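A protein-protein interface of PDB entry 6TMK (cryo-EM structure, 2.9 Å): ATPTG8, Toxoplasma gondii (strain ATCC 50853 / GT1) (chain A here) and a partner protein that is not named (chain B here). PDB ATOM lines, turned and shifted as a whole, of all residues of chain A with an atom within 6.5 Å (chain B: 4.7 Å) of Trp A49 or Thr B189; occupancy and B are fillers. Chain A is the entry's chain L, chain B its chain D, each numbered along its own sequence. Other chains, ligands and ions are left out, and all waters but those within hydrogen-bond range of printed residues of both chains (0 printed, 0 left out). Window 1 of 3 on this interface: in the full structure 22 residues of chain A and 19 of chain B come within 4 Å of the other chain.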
ATOM      1  N   THR A   2      35.672  14.760  28.292  1.00  0.00           N
ATOM      2  CA  THR A   2      36.238  13.506  27.813  1.00  0.00           C
ATOM      3  C   THR A   2      35.167  12.642  27.161  1.00  0.00           C
ATOM      4  O   THR A   2      33.978  12.801  27.425  1.00  0.00           O
ATOM      5  CB  THR A   2      36.902  12.720  28.956  1.00  0.00           C
ATOM      6  OG1 THR A   2      37.614  11.599  28.417  1.00  0.00           O
ATOM      7  CG2 THR A   2      35.859  12.236  29.956  1.00  0.00           C
ATOM      8  N   GLU A  44      20.178  22.043  16.675  1.00  0.00           N
ATOM      9  CA  GLU A  44      20.153  23.493  16.854  1.00  0.00           C
ATOM     10  C   GLU A  44      21.005  23.914  18.048  1.00  0.00           C
ATOM     11  O   GLU A  44      21.796  24.868  17.968  1.00  0.00           O
ATOM     12  CB  GLU A  44      18.716  23.970  17.030  1.00  0.00           C
ATOM     13  CG  GLU A  44      17.970  24.150  15.736  1.00  0.00           C
ATOM     14  CD  GLU A  44      16.477  24.309  15.938  1.00  0.00           C
ATOM     15  OE1 GLU A  44      15.840  23.362  16.443  1.00  0.00           O
ATOM     16  OE2 GLU A  44      15.940  25.381  15.589  1.00  0.00           O
ATOM     17  N   LEU A  45      20.836  23.223  19.175  1.00  0.00           N
ATOM     18  CA  LEU A  45      21.623  23.535  20.361  1.00  0.00           C
ATOM     19  C   LEU A  45      23.113  23.396  20.093  1.00  0.00           C
ATOM     20  O   LEU A  45      23.913  24.214  20.559  1.00  0.00           O
ATOM     21  CB  LEU A  45      21.218  22.626  21.513  1.00  0.00           C
ATOM     22  CG  LEU A  45      19.984  23.008  22.313  1.00  0.00           C
ATOM     23  CD1 LEU A  45      19.507  21.817  23.097  1.00  0.00           C
ATOM     24  CD2 LEU A  45      20.298  24.155  23.227  1.00  0.00           C
ATOM     25  N   LYS A  46      23.508  22.352  19.366  1.00  0.00           N
ATOM     26  CA  LYS A  46      24.912  22.159  19.048  1.00  0.00           C
ATOM     27  C   LYS A  46      25.446  23.300  18.204  1.00  0.00           C
ATOM     28  O   LYS A  46      26.561  23.778  18.430  1.00  0.00           O
ATOM     29  CB  LYS A  46      25.106  20.835  18.326  1.00  0.00           C
ATOM     30  CG  LYS A  46      26.539  20.428  18.210  1.00  0.00           C
ATOM     31  CD  LYS A  46      26.719  19.301  17.246  1.00  0.00           C
ATOM     32  CE  LYS A  46      28.171  19.047  16.989  1.00  0.00           C
ATOM     33  NZ  LYS A  46      28.416  17.699  16.471  1.00  0.00           N
ATOM     34  N   ASP A  47      24.671  23.747  17.222  1.00  0.00           N
ATOM     35  CA  ASP A  47      25.126  24.854  16.392  1.00  0.00           C
ATOM     36  C   ASP A  47      25.367  26.089  17.245  1.00  0.00           C
ATOM     37  O   ASP A  47      26.433  26.718  17.172  1.00  0.00           O
ATOM     38  CB  ASP A  47      24.121  25.138  15.281  1.00  0.00           C
ATOM     39  CG  ASP A  47      24.780  25.669  14.022  1.00  0.00           C
ATOM     40  OD1 ASP A  47      25.849  26.305  14.131  1.00  0.00           O
ATOM     41  OD2 ASP A  47      24.235  25.450  12.921  1.00  0.00           O
ATOM     42  N   TRP A  48      24.392  26.434  18.086  1.00  0.00           N
ATOM     43  CA  TRP A  48      24.559  27.582  18.969  1.00  0.00           C
ATOM     44  C   TRP A  48      25.800  27.437  19.836  1.00  0.00           C
ATOM     45  O   TRP A  48      26.642  28.342  19.895  1.00  0.00           O
ATOM     46  CB  TRP A  48      23.323  27.758  19.848  1.00  0.00           C
ATOM     47  CG  TRP A  48      23.551  28.702  20.974  1.00  0.00           C
ATOM     48  CD1 TRP A  48      23.506  30.054  20.920  1.00  0.00           C
ATOM     49  CD2 TRP A  48      23.871  28.366  22.328  1.00  0.00           C
ATOM     50  NE1 TRP A  48      23.777  30.588  22.153  1.00  0.00           N
ATOM     51  CE2 TRP A  48      24.004  29.568  23.034  1.00  0.00           C
ATOM     52  CE3 TRP A  48      24.058  27.165  23.010  1.00  0.00           C
ATOM     53  CZ2 TRP A  48      24.313  29.605  24.381  1.00  0.00           C
ATOM     54  CZ3 TRP A  48      24.365  27.209  24.344  1.00  0.00           C
ATOM     55  CH2 TRP A  48      24.491  28.416  25.015  1.00  0.00           C
ATOM     56  N   TRP A  49      25.921  26.309  20.528  1.00  0.00           N
ATOM     57  CA  TRP A  49      27.001  26.139  21.486  1.00  0.00           C
ATOM     58  C   TRP A  49      28.358  26.196  20.805  1.00  0.00           C
ATOM     59  O   TRP A  49      29.289  26.827  21.317  1.00  0.00           O
ATOM     60  CB  TRP A  49      26.818  24.816  22.217  1.00  0.00           C
ATOM     61  CG  TRP A  49      27.689  24.639  23.393  1.00  0.00           C
ATOM     62  CD1 TRP A  49      27.423  25.019  24.663  1.00  0.00           C
ATOM     63  CD2 TRP A  49      28.972  24.019  23.420  1.00  0.00           C
ATOM     64  NE1 TRP A  49      28.459  24.683  25.485  1.00  0.00           N
ATOM     65  CE2 TRP A  49      29.426  24.066  24.743  1.00  0.00           C
ATOM     66  CE3 TRP A  49      29.782  23.428  22.453  1.00  0.00           C
ATOM     67  CZ2 TRP A  49      30.652  23.550  25.122  1.00  0.00           C
ATOM     68  CZ3 TRP A  49      30.991  22.923  22.832  1.00  0.00           C
ATOM     69  CH2 TRP A  49      31.416  22.983  24.151  1.00  0.00           C
ATOM     70  N   MET A  50      28.495  25.553  19.649  1.00  0.00           N
ATOM     71  CA  MET A  50      29.796  25.495  19.006  1.00  0.00           C
ATOM     72  C   MET A  50      30.182  26.847  18.430  1.00  0.00           C
ATOM     73  O   MET A  50      31.347  27.253  18.521  1.00  0.00           O
ATOM     74  CB  MET A  50      29.800  24.426  17.920  1.00  0.00           C
ATOM     75  CG  MET A  50      29.562  23.030  18.426  1.00  0.00           C
ATOM     76  SD  MET A  50      31.026  22.287  19.138  1.00  0.00           S
ATOM     77  CE  MET A  50      31.779  21.695  17.642  1.00  0.00           C
ATOM     78  N   SER A  51      29.223  27.575  17.856  1.00  0.00           N
ATOM     79  CA  SER A  51      29.527  28.914  17.377  1.00  0.00           C
ATOM     80  C   SER A  51      29.961  29.809  18.528  1.00  0.00           C
ATOM     81  O   SER A  51      30.962  30.533  18.431  1.00  0.00           O
ATOM     82  CB  SER A  51      28.313  29.495  16.659  1.00  0.00           C
ATOM     83  OG  SER A  51      27.765  28.562  15.751  1.00  0.00           O
ATOM     84  N   ARG A  52      29.230  29.749  19.642  1.00  0.00           N
ATOM     85  CA  ARG A  52      29.558  30.568  20.800  1.00  0.00           C
ATOM     86  C   ARG A  52      30.950  30.238  21.325  1.00  0.00           C
ATOM     87  O   ARG A  52      31.756  31.136  21.598  1.00  0.00           O
ATOM     88  CB  ARG A  52      28.493  30.347  21.874  1.00  0.00           C
ATOM     89  CG  ARG A  52      28.529  31.282  23.047  1.00  0.00           C
ATOM     90  CD  ARG A  52      28.066  32.669  22.677  1.00  0.00           C
ATOM     91  NE  ARG A  52      28.310  33.617  23.758  1.00  0.00           N
ATOM     92  CZ  ARG A  52      27.369  34.197  24.490  1.00  0.00           C
ATOM     93  NH1 ARG A  52      27.717  35.036  25.445  1.00  0.00           N
ATOM     94  NH2 ARG A  52      26.088  33.955  24.276  1.00  0.00           N
ATOM     95  N   LYS A  53      31.250  28.948  21.460  1.00  0.00           N
ATOM     96  CA  LYS A  53      32.546  28.518  21.968  1.00  0.00           C
ATOM     97  C   LYS A  53      33.679  28.982  21.063  1.00  0.00           C
ATOM     98  O   LYS A  53      34.688  29.525  21.535  1.00  0.00           O
ATOM     99  CB  LYS A  53      32.533  26.997  22.105  1.00  0.00           C
ATOM    100  CG  LYS A  53      33.772  26.370  22.658  1.00  0.00           C
ATOM    101  CD  LYS A  53      33.846  26.549  24.136  1.00  0.00           C
ATOM    102  CE  LYS A  53      35.152  26.045  24.681  1.00  0.00           C
ATOM    103  NZ  LYS A  53      35.186  24.582  24.652  1.00  0.00           N
ATOM    104  N   ILE A  54      33.537  28.767  19.753  1.00  0.00           N
ATOM    105  CA  ILE A  54      34.607  29.118  18.829  1.00  0.00           C
ATOM    106  C   ILE A  54      34.846  30.618  18.844  1.00  0.00           C
ATOM    107  O   ILE A  54      35.994  31.077  18.856  1.00  0.00           O
ATOM    108  CB  ILE A  54      34.292  28.608  17.413  1.00  0.00           C
ATOM    109  CG1 ILE A  54      34.276  27.091  17.384  1.00  0.00           C
ATOM    110  CG2 ILE A  54      35.329  29.087  16.436  1.00  0.00           C
ATOM    111  CD1 ILE A  54      33.483  26.531  16.272  1.00  0.00           C
ATOM    112  N   ASP B 185      38.200  18.029  19.667  1.00  0.00           N
ATOM    113  CA  ASP B 185      38.068  18.550  21.023  1.00  0.00           C
ATOM    114  C   ASP B 185      36.686  19.153  21.242  1.00  0.00           C
ATOM    115  O   ASP B 185      36.015  18.865  22.241  1.00  0.00           O
ATOM    116  CB  ASP B 185      39.156  19.588  21.285  1.00  0.00           C
ATOM    117  CG  ASP B 185      40.486  18.964  21.654  1.00  0.00           C
ATOM    118  OD1 ASP B 185      40.512  17.774  22.034  1.00  0.00           O
ATOM    119  OD2 ASP B 185      41.514  19.667  21.559  1.00  0.00           O
ATOM    120  N   LEU B 186      36.238  19.985  20.301  1.00  0.00           N
ATOM    121  CA  LEU B 186      34.976  20.693  20.473  1.00  0.00           C
ATOM    122  C   LEU B 186      33.804  19.724  20.518  1.00  0.00           C
ATOM    123  O   LEU B 186      32.916  19.842  21.370  1.00  0.00           O
ATOM    124  CB  LEU B 186      34.785  21.706  19.348  1.00  0.00           C
ATOM    125  CG  LEU B 186      35.711  22.914  19.334  1.00  0.00           C
ATOM    126  CD1 LEU B 186      35.766  23.512  17.954  1.00  0.00           C
ATOM    127  CD2 LEU B 186      35.239  23.932  20.329  1.00  0.00           C
ATOM    128  N   GLU B 187      33.776  18.762  19.600  1.00  0.00           N
ATOM    129  CA  GLU B 187      32.638  17.856  19.526  1.00  0.00           C
ATOM    130  C   GLU B 187      32.594  16.928  20.735  1.00  0.00           C
ATOM    131  O   GLU B 187      31.513  16.630  21.264  1.00  0.00           O
ATOM    132  CB  GLU B 187      32.701  17.064  18.227  1.00  0.00           C
ATOM    133  CG  GLU B 187      32.407  17.906  17.011  1.00  0.00           C
ATOM    134  CD  GLU B 187      32.464  17.130  15.715  1.00  0.00           C
ATOM    135  OE1 GLU B 187      31.427  17.048  15.024  1.00  0.00           O
ATOM    136  OE2 GLU B 187      33.546  16.604  15.381  1.00  0.00           O
ATOM    137  N   THR B 188      33.756  16.476  21.201  1.00  0.00           N
ATOM    138  CA  THR B 188      33.800  15.673  22.417  1.00  0.00           C
ATOM    139  C   THR B 188      33.302  16.464  23.621  1.00  0.00           C
ATOM    140  O   THR B 188      32.515  15.955  24.434  1.00  0.00           O
ATOM    141  CB  THR B 188      35.225  15.179  22.640  1.00  0.00           C
ATOM    142  OG1 THR B 188      35.551  14.206  21.643  1.00  0.00           O
ATOM    143  CG2 THR B 188      35.379  14.567  24.000  1.00  0.00           C
ATOM    144  N   THR B 189      33.749  17.715  23.753  1.00  0.00           N
ATOM    145  CA  THR B 189      33.282  18.554  24.846  1.00  0.00           C
ATOM    146  C   THR B 189      31.782  18.789  24.759  1.00  0.00           C
ATOM    147  O   THR B 189      31.099  18.853  25.785  1.00  0.00           O
ATOM    148  CB  THR B 189      34.043  19.874  24.846  1.00  0.00           C
ATOM    149  OG1 THR B 189      35.445  19.611  24.924  1.00  0.00           O
ATOM    150  CG2 THR B 189      33.636  20.723  26.011  1.00  0.00           C
ATOM    151  N   TRP B 190      31.246  18.900  23.545  1.00  0.00           N
ATOM    152  CA  TRP B 190      29.808  19.088  23.393  1.00  0.00           C
ATOM    153  C   TRP B 190      29.043  17.857  23.844  1.00  0.00           C
ATOM    154  O   TRP B 190      28.010  17.973  24.511  1.00  0.00           O
ATOM    155  CB  TRP B 190      29.456  19.413  21.948  1.00  0.00           C
ATOM    156  CG  TRP B 190      28.031  19.122  21.640  1.00  0.00           C
ATOM    157  CD1 TRP B 190      27.553  18.122  20.860  1.00  0.00           C
ATOM    158  CD2 TRP B 190      26.892  19.834  22.121  1.00  0.00           C
ATOM    159  NE1 TRP B 190      26.186  18.162  20.825  1.00  0.00           N
ATOM    160  CE2 TRP B 190      25.756  19.209  21.591  1.00  0.00           C
ATOM    161  CE3 TRP B 190      26.722  20.939  22.948  1.00  0.00           C
ATOM    162  CZ2 TRP B 190      24.474  19.655  21.858  1.00  0.00           C
ATOM    163  CZ3 TRP B 190      25.456  21.374  23.209  1.00  0.00           C
ATOM    164  CH2 TRP B 190      24.347  20.738  22.669  1.00  0.00           C
ATOM    165  N   GLU B 191      29.515  16.673  23.469  1.00  0.00           N
ATOM    166  CA  GLU B 191      28.857  15.451  23.916  1.00  0.00           C
ATOM    167  C   GLU B 191      28.846  15.362  25.437  1.00  0.00           C
ATOM    168  O   GLU B 191      27.805  15.089  26.051  1.00  0.00           O
ATOM    169  CB  GLU B 191      29.561  14.243  23.309  1.00  0.00           C
ATOM    170  CG  GLU B 191      29.377  14.120  21.827  1.00  0.00           C
ATOM    171  CD  GLU B 191      30.309  13.098  21.211  1.00  0.00           C
ATOM    172  OE1 GLU B 191      31.059  12.446  21.968  1.00  0.00           O
ATOM    173  OE2 GLU B 191      30.298  12.946  19.971  1.00  0.00           O
ATOM    174  N   GLU B 192      29.996  15.611  26.063  1.00  0.00           N
ATOM    175  CA  GLU B 192      30.065  15.573  27.519  1.00  0.00           C
ATOM    176  C   GLU B 192      29.127  16.598  28.149  1.00  0.00           C
ATOM    177  O   GLU B 192      28.395  16.289  29.103  1.00  0.00           O
ATOM    178  CB  GLU B 192      31.501  15.817  27.967  1.00  0.00           C
ATOM    179  CG  GLU B 192      31.771  15.492  29.407  1.00  0.00           C
ATOM    180  CD  GLU B 192      33.215  15.723  29.777  1.00  0.00           C
ATOM    181  OE1 GLU B 192      33.936  16.342  28.967  1.00  0.00           O
ATOM    182  OE2 GLU B 192      33.630  15.285  30.870  1.00  0.00           O
ATOM    183  N   ALA B 193      29.144  17.828  27.636  1.00  0.00           N
ATOM    184  CA  ALA B 193      28.310  18.882  28.191  1.00  0.00           C
ATOM    185  C   ALA B 193      26.837  18.543  28.071  1.00  0.00           C
ATOM    186  O   ALA B 193      26.067  18.754  29.012  1.00  0.00           O
ATOM    187  CB  ALA B 193      28.607  20.200  27.481  1.00  0.00           C
ATOM    188  N   LEU B 206      25.593  23.508  30.621  1.00  0.00           N
ATOM    189  CA  LEU B 206      26.036  23.776  29.260  1.00  0.00           C
ATOM    190  C   LEU B 206      26.838  25.063  29.185  1.00  0.00           C
ATOM    191  O   LEU B 206      27.888  25.118  28.538  1.00  0.00           O
ATOM    192  CB  LEU B 206      24.825  23.881  28.336  1.00  0.00           C
ATOM    193  CG  LEU B 206      24.257  22.658  27.635  1.00  0.00           C
ATOM    194  CD1 LEU B 206      23.235  23.113  26.633  1.00  0.00           C
ATOM    195  CD2 LEU B 206      25.316  21.861  26.949  1.00  0.00           C
ATOM    196  N   TYR B 209      30.329  24.642  30.541  1.00  0.00           N
ATOM    197  CA  TYR B 209      31.258  23.928  29.670  1.00  0.00           C
ATOM    198  C   TYR B 209      31.835  24.795  28.560  1.00  0.00           C
ATOM    199  O   TYR B 209      32.621  24.287  27.754  1.00  0.00           O
ATOM    200  CB  TYR B 209      30.601  22.680  29.080  1.00  0.00           C
ATOM    201  CG  TYR B 209      30.465  21.543  30.061  1.00  0.00           C
ATOM    202  CD1 TYR B 209      31.555  20.745  30.350  1.00  0.00           C
ATOM    203  CD2 TYR B 209      29.277  21.282  30.714  1.00  0.00           C
ATOM    204  CE1 TYR B 209      31.465  19.709  31.236  1.00  0.00           C
ATOM    205  CE2 TYR B 209      29.180  20.243  31.610  1.00  0.00           C
ATOM    206  CZ  TYR B 209      30.282  19.466  31.874  1.00  0.00           C
ATOM    207  OH  TYR B 209      30.204  18.427  32.767  1.00  0.00           O
ATOM    208  N   LEU B 210      31.485  26.079  28.494  1.00  0.00           N
ATOM    209  CA  LEU B 210      32.054  26.955  27.481  1.00  0.00           C
ATOM    210  C   LEU B 210      33.468  27.404  27.811  1.00  0.00           C
ATOM    211  O   LEU B 210      34.102  28.053  26.974  1.00  0.00           O
ATOM    212  CB  LEU B 210      31.186  28.193  27.286  1.00  0.00           C
ATOM    213  CG  LEU B 210      29.814  28.006  26.658  1.00  0.00           C
ATOM    214  CD1 LEU B 210      29.002  29.250  26.818  1.00  0.00           C
ATOM    215  CD2 LEU B 210      29.972  27.697  25.203  1.00  0.00           C
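OE1 of Glu B192 lies within hydrogen-bond range of N of Thr A2 (2.4 Å). The side-chain amino group (NZ) of Lys A46 lies within salt-bridge range of the side-chain carboxylate (OE1) of Glu B187, 3.4 Å away. NE1 of Trp A49 lies within hydrogen-bond range of O of Leu B206 (3.1 Å).
O of Asp B185 is in hydrogen-bond range of OG1 of Thr B189 (2.8 Å).
Among the printed residues, merely in contact across the chains: Lys A53 with Leu B210 (3.2 Å), Trp A49 with Tyr B209 (3.4 Å), Trp A49 with Leu B210 (3.4 Å), Met A50 with Leu B186 (3.5 Å), Lys A46 with Trp B190 (3.5 Å), Trp A49 with Thr B189 (3.7 Å), Lys A53 with Leu B186 (3.7 Å), Thr A2 with Thr B188 (3.7 Å), Trp A49 with Trp B190 (3.8 Å), Leu A45 with Trp B190 (3.8 Å), Met A50 with Glu B187 (3.9 Å), Trp A49 with Leu B186 (3.9 Å) and Ile A54 with Leu B186 (3.9 Å).
Of the printed residues of chain B, Thr A2 touches Thr B188 (3.7 Å) and Glu B192 (2.4 Å). Of chain B, only Leu B186 (3.9 Å), Thr B189 (3.7 Å), Trp B190 (3.8 Å), Leu B206 (3.1 Å), Tyr B209 (3.4 Å) and Leu B210 (3.4 Å) come within 4 Å of Trp A49. Thr B189 touches just one residue of chain A: Trp A49. Of the printed residues of chain A, Tyr B209 touches Trp A49. The nearest residue of chain B that does not touch Trp A49 is Ala B193 (4.6 Å). The nearest residue of chain A that does not touch Thr B189 is Lys A53 (4.4 Å). The nearest printed residue of chain A that does not touch Thr B188 is Met A50 (6.6 Å).
Hydrophobic or aromatic side chains of chain B that line the printed part of chain A: Leu B186, Trp B190 and Leu B210. Of the 12 printed residues of chain A, 7 touch a printed residue of chain B. Hydrophobic or aromatic side chains of chain A that line the printed part of chain B: Leu A45, Trp A49, Met A50 and Ile A54. Along chain A the printed residues that touch a printed residue of chain B span positions 2 to 54. Among the printed residues, Asp or Glu carboxylates within 4 Å of a Lys or Arg side-chain nitrogen of the other chain: Lys A46 with Glu B187 (3.4 Å).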
